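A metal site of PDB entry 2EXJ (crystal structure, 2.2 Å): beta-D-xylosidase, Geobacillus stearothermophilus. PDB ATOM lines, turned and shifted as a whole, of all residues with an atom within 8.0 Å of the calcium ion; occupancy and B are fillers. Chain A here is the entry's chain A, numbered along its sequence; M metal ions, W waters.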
ATOM      1  N   LYS A 331      23.847  35.613  -4.753  1.00  0.00           N
ATOM      2  CA  LYS A 331      24.191  34.696  -5.843  1.00  0.00           C
ATOM      3  C   LYS A 331      24.347  33.284  -5.277  1.00  0.00           C
ATOM      4  O   LYS A 331      25.333  32.976  -4.648  1.00  0.00           O
ATOM      5  CB  LYS A 331      25.456  35.135  -6.555  1.00  0.00           C
ATOM      6  CG  LYS A 331      25.756  34.351  -7.829  1.00  0.00           C
ATOM      7  CD  LYS A 331      26.921  34.979  -8.586  1.00  0.00           C
ATOM      8  CE  LYS A 331      27.456  34.041  -9.641  1.00  0.00           C
ATOM      9  NZ  LYS A 331      28.638  34.646 -10.402  1.00  0.00           N
ATOM     10  N   ASP A 332      23.342  32.431  -5.529  1.00  0.00           N
ATOM     11  CA  ASP A 332      23.269  31.101  -4.939  1.00  0.00           C
ATOM     12  C   ASP A 332      23.942  30.179  -5.923  1.00  0.00           C
ATOM     13  O   ASP A 332      23.423  29.929  -7.004  1.00  0.00           O
ATOM     14  CB  ASP A 332      21.826  30.732  -4.688  1.00  0.00           C
ATOM     15  CG  ASP A 332      21.624  29.317  -4.127  1.00  0.00           C
ATOM     16  OD1 ASP A 332      22.488  28.424  -4.305  1.00  0.00           O
ATOM     17  OD2 ASP A 332      20.542  29.113  -3.519  1.00  0.00           O
ATOM     18  N   ASP A 333      25.130  29.700  -5.551  1.00  0.00           N
ATOM     19  CA  ASP A 333      25.960  28.895  -6.483  1.00  0.00           C
ATOM     20  C   ASP A 333      25.653  27.429  -6.511  1.00  0.00           C
ATOM     21  O   ASP A 333      26.297  26.676  -7.232  1.00  0.00           O
ATOM     22  CB  ASP A 333      27.443  29.086  -6.182  1.00  0.00           C
ATOM     23  CG  ASP A 333      28.122  29.894  -7.231  1.00  0.00           C
ATOM     24  OD1 ASP A 333      28.480  29.323  -8.318  1.00  0.00           O
ATOM     25  OD2 ASP A 333      28.301  31.121  -6.979  1.00  0.00           O
ATOM     26  N   PHE A 334      24.630  27.021  -5.759  1.00  0.00           N
ATOM     27  CA  PHE A 334      24.166  25.617  -5.706  1.00  0.00           C
ATOM     28  C   PHE A 334      25.244  24.767  -5.065  1.00  0.00           C
ATOM     29  O   PHE A 334      25.659  23.726  -5.597  1.00  0.00           O
ATOM     30  CB  PHE A 334      23.684  25.087  -7.074  1.00  0.00           C
ATOM     31  CG  PHE A 334      22.468  25.825  -7.585  1.00  0.00           C
ATOM     32  CD1 PHE A 334      21.343  26.004  -6.777  1.00  0.00           C
ATOM     33  CD2 PHE A 334      22.449  26.384  -8.855  1.00  0.00           C
ATOM     34  CE1 PHE A 334      20.212  26.699  -7.245  1.00  0.00           C
ATOM     35  CE2 PHE A 334      21.338  27.079  -9.343  1.00  0.00           C
ATOM     36  CZ  PHE A 334      20.223  27.256  -8.535  1.00  0.00           C
ATOM     37  N   ASP A 335      25.695  25.235  -3.905  1.00  0.00           N
ATOM     38  CA  ASP A 335      26.842  24.684  -3.218  1.00  0.00           C
ATOM     39  C   ASP A 335      26.438  23.661  -2.191  1.00  0.00           C
ATOM     40  O   ASP A 335      27.230  22.808  -1.828  1.00  0.00           O
ATOM     41  CB  ASP A 335      27.640  25.797  -2.507  1.00  0.00           C
ATOM     42  CG  ASP A 335      28.427  26.677  -3.469  1.00  0.00           C
ATOM     43  OD1 ASP A 335      28.894  26.193  -4.526  1.00  0.00           O
ATOM     44  OD2 ASP A 335      28.584  27.875  -3.119  1.00  0.00           O
ATOM     45  N   ARG A 360      25.596  16.942 -11.400  1.00  0.00           N
ATOM     46  CA  ARG A 360      26.728  17.797 -11.785  1.00  0.00           C
ATOM     47  C   ARG A 360      27.099  18.716 -10.658  1.00  0.00           C
ATOM     48  O   ARG A 360      26.349  19.640 -10.327  1.00  0.00           O
ATOM     49  CB  ARG A 360      26.481  18.606 -13.060  1.00  0.00           C
ATOM     50  CG  ARG A 360      27.767  19.150 -13.740  1.00  0.00           C
ATOM     51  CD  ARG A 360      27.446  19.845 -15.058  1.00  0.00           C
ATOM     52  NE  ARG A 360      28.491  20.781 -15.462  1.00  0.00           N
ATOM     53  CZ  ARG A 360      28.457  21.547 -16.555  1.00  0.00           C
ATOM     54  NH1 ARG A 360      27.430  21.520 -17.397  1.00  0.00           N
ATOM     55  NH2 ARG A 360      29.468  22.376 -16.790  1.00  0.00           N
ATOM     56  N   PRO A 361      28.297  18.517 -10.079  1.00  0.00           N
ATOM     57  CA  PRO A 361      28.666  19.240  -8.855  1.00  0.00           C
ATOM     58  C   PRO A 361      28.527  20.763  -9.014  1.00  0.00           C
ATOM     59  O   PRO A 361      28.846  21.333 -10.066  1.00  0.00           O
ATOM     60  CB  PRO A 361      30.121  18.793  -8.584  1.00  0.00           C
ATOM     61  CG  PRO A 361      30.314  17.548  -9.359  1.00  0.00           C
ATOM     62  CD  PRO A 361      29.361  17.612 -10.554  1.00  0.00           C
ATOM     63  N   GLY A 362      27.999  21.416  -7.995  1.00  0.00           N
ATOM     64  CA  GLY A 362      27.759  22.862  -8.030  1.00  0.00           C
ATOM     65  C   GLY A 362      26.764  23.375  -9.067  1.00  0.00           C
ATOM     66  O   GLY A 362      26.789  24.560  -9.402  1.00  0.00           O
ATOM     67  N   HIS A 363      25.888  22.494  -9.536  1.00  0.00           N
ATOM     68  CA  HIS A 363      24.804  22.834 -10.442  1.00  0.00           C
ATOM     69  C   HIS A 363      23.498  22.227  -9.972  1.00  0.00           C
ATOM     70  O   HIS A 363      23.454  21.041  -9.596  1.00  0.00           O
ATOM     71  CB  HIS A 363      25.087  22.252 -11.831  1.00  0.00           C
ATOM     72  CG  HIS A 363      26.237  22.897 -12.536  1.00  0.00           C
ATOM     73  ND1 HIS A 363      27.552  22.710 -12.159  1.00  0.00           N
ATOM     74  CD2 HIS A 363      26.274  23.709 -13.613  1.00  0.00           C
ATOM     75  CE1 HIS A 363      28.338  23.386 -12.964  1.00  0.00           C
ATOM     76  NE2 HIS A 363      27.591  23.999 -13.862  1.00  0.00           N
ATOM     77  N   LEU A 364      22.427  22.997 -10.058  1.00  0.00           N
ATOM     78  CA  LEU A 364      21.107  22.375 -10.103  1.00  0.00           C
ATOM     79  C   LEU A 364      20.877  21.831 -11.498  1.00  0.00           C
ATOM     80  O   LEU A 364      20.933  22.569 -12.505  1.00  0.00           O
ATOM     81  CB  LEU A 364      19.992  23.356  -9.748  1.00  0.00           C
ATOM     82  CG  LEU A 364      18.577  22.799  -9.925  1.00  0.00           C
ATOM     83  CD1 LEU A 364      18.306  21.668  -8.894  1.00  0.00           C
ATOM     84  CD2 LEU A 364      17.631  23.967  -9.772  1.00  0.00           C
ATOM     85  N   LYS A 395      22.475  31.026 -15.045  1.00  0.00           N
ATOM     86  CA  LYS A 395      23.487  30.665 -16.036  1.00  0.00           C
ATOM     87  C   LYS A 395      23.367  29.165 -16.323  1.00  0.00           C
ATOM     88  O   LYS A 395      23.522  28.328 -15.433  1.00  0.00           O
ATOM     89  CB  LYS A 395      24.872  31.042 -15.508  1.00  0.00           C
ATOM     90  CG  LYS A 395      26.048  30.410 -16.213  1.00  0.00           C
ATOM     91  CD  LYS A 395      27.311  30.606 -15.363  1.00  0.00           C
ATOM     92  CE  LYS A 395      28.470  29.844 -15.903  1.00  0.00           C
ATOM     93  NZ  LYS A 395      29.619  30.008 -14.945  1.00  0.00           N
ATOM     94  N   TYR A 460      27.536  28.027 -21.952  1.00  0.00           N
ATOM     95  CA  TYR A 460      26.583  28.609 -21.016  1.00  0.00           C
ATOM     96  C   TYR A 460      25.877  29.845 -21.543  1.00  0.00           C
ATOM     97  O   TYR A 460      26.502  30.748 -22.106  1.00  0.00           O
ATOM     98  CB  TYR A 460      27.319  28.998 -19.740  1.00  0.00           C
ATOM     99  CG  TYR A 460      27.637  27.877 -18.797  1.00  0.00           C
ATOM    100  CD1 TYR A 460      26.624  27.207 -18.098  1.00  0.00           C
ATOM    101  CD2 TYR A 460      28.957  27.531 -18.542  1.00  0.00           C
ATOM    102  CE1 TYR A 460      26.928  26.184 -17.174  1.00  0.00           C
ATOM    103  CE2 TYR A 460      29.281  26.505 -17.628  1.00  0.00           C
ATOM    104  CZ  TYR A 460      28.248  25.841 -16.948  1.00  0.00           C
ATOM    105  OH  TYR A 460      28.583  24.826 -16.053  1.00  0.00           O
ATOM    106  N   PHE A 527      22.030  24.300 -14.282  1.00  0.00           N
ATOM    107  CA  PHE A 527      22.036  25.699 -13.824  1.00  0.00           C
ATOM    108  C   PHE A 527      23.194  25.913 -12.869  1.00  0.00           C
ATOM    109  O   PHE A 527      23.222  25.333 -11.783  1.00  0.00           O
ATOM    110  CB  PHE A 527      20.701  26.088 -13.146  1.00  0.00           C
ATOM    111  CG  PHE A 527      19.508  26.010 -14.073  1.00  0.00           C
ATOM    112  CD1 PHE A 527      19.051  27.147 -14.759  1.00  0.00           C
ATOM    113  CD2 PHE A 527      18.855  24.798 -14.285  1.00  0.00           C
ATOM    114  CE1 PHE A 527      17.988  27.051 -15.659  1.00  0.00           C
ATOM    115  CE2 PHE A 527      17.780  24.696 -15.196  1.00  0.00           C
ATOM    116  CZ  PHE A 527      17.345  25.838 -15.882  1.00  0.00           C
ATOM    117  N   ASP A 528      24.148  26.742 -13.265  1.00  0.00           N
ATOM    118  CA  ASP A 528      25.320  26.950 -12.453  1.00  0.00           C
ATOM    119  C   ASP A 528      24.991  27.739 -11.178  1.00  0.00           C
ATOM    120  O   ASP A 528      25.474  27.420 -10.088  1.00  0.00           O
ATOM    121  CB  ASP A 528      26.446  27.593 -13.268  1.00  0.00           C
ATOM    122  CG  ASP A 528      27.736  27.730 -12.477  1.00  0.00           C
ATOM    123  OD1 ASP A 528      28.476  28.655 -12.817  1.00  0.00           O
ATOM    124  OD2 ASP A 528      28.005  26.943 -11.502  1.00  0.00           O
ATOM    125  N   TYR A 529      24.136  28.751 -11.308  1.00  0.00           N
ATOM    126  CA  TYR A 529      23.731  29.537 -10.144  1.00  0.00           C
ATOM    127  C   TYR A 529      22.367  30.202 -10.419  1.00  0.00           C
ATOM    128  O   TYR A 529      21.880  30.190 -11.562  1.00  0.00           O
ATOM    129  CB  TYR A 529      24.816  30.577  -9.790  1.00  0.00           C
ATOM    130  CG  TYR A 529      24.970  31.680 -10.823  1.00  0.00           C
ATOM    131  CD1 TYR A 529      24.035  32.738 -10.875  1.00  0.00           C
ATOM    132  CD2 TYR A 529      26.008  31.664 -11.740  1.00  0.00           C
ATOM    133  CE1 TYR A 529      24.142  33.739 -11.849  1.00  0.00           C
ATOM    134  CE2 TYR A 529      26.141  32.689 -12.692  1.00  0.00           C
ATOM    135  CZ  TYR A 529      25.211  33.714 -12.738  1.00  0.00           C
ATOM    136  OH  TYR A 529      25.350  34.715 -13.673  1.00  0.00           O
ATOM    137  N   PHE A 530      21.753  30.715  -9.366  1.00  0.00           N
ATOM    138  CA  PHE A 530      20.529  31.535  -9.453  1.00  0.00           C
ATOM    139  C   PHE A 530      20.717  32.718  -8.521  1.00  0.00           C
ATOM    140  O   PHE A 530      20.985  32.532  -7.340  1.00  0.00           O
ATOM    141  CB  PHE A 530      19.255  30.786  -9.042  1.00  0.00           C
ATOM    142  CG  PHE A 530      17.983  31.597  -9.230  1.00  0.00           C
ATOM    143  CD1 PHE A 530      17.326  31.619 -10.466  1.00  0.00           C
ATOM    144  CD2 PHE A 530      17.455  32.351  -8.188  1.00  0.00           C
ATOM    145  CE1 PHE A 530      16.144  32.361 -10.644  1.00  0.00           C
ATOM    146  CE2 PHE A 530      16.276  33.112  -8.364  1.00  0.00           C
ATOM    147  CZ  PHE A 530      15.623  33.104  -9.614  1.00  0.00           C
HETATM  148 CA    CA M   1      27.688  26.600  -9.211  1.00  0.00          CA
HETATM  149  O   HOH W   1      29.205  25.915  -7.096  1.00  0.00           O
HETATM  150  O   HOH W   2      29.872  25.669  -9.810  1.00  0.00           O
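The calcium ion is bound by the backbone carbonyl oxygen of Gly 362, the side-chain carboxylate of Asp 528, the backbone carbonyl oxygen of Asp 333, water W2, the backbone carbonyl oxygen of Asp 528 and water W1.
The calcium ion has six donor atoms within binding distance.
Slightly farther from the calcium ion lies the side-chain carboxylate (OD1) of Asp 333 (3.0 Å).
The nearest printed residue that does not touch the calcium ion is His 363 (4.5 Å).
OD1 of Asp 528 lies within salt-bridge range of NZ of Lys 395.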
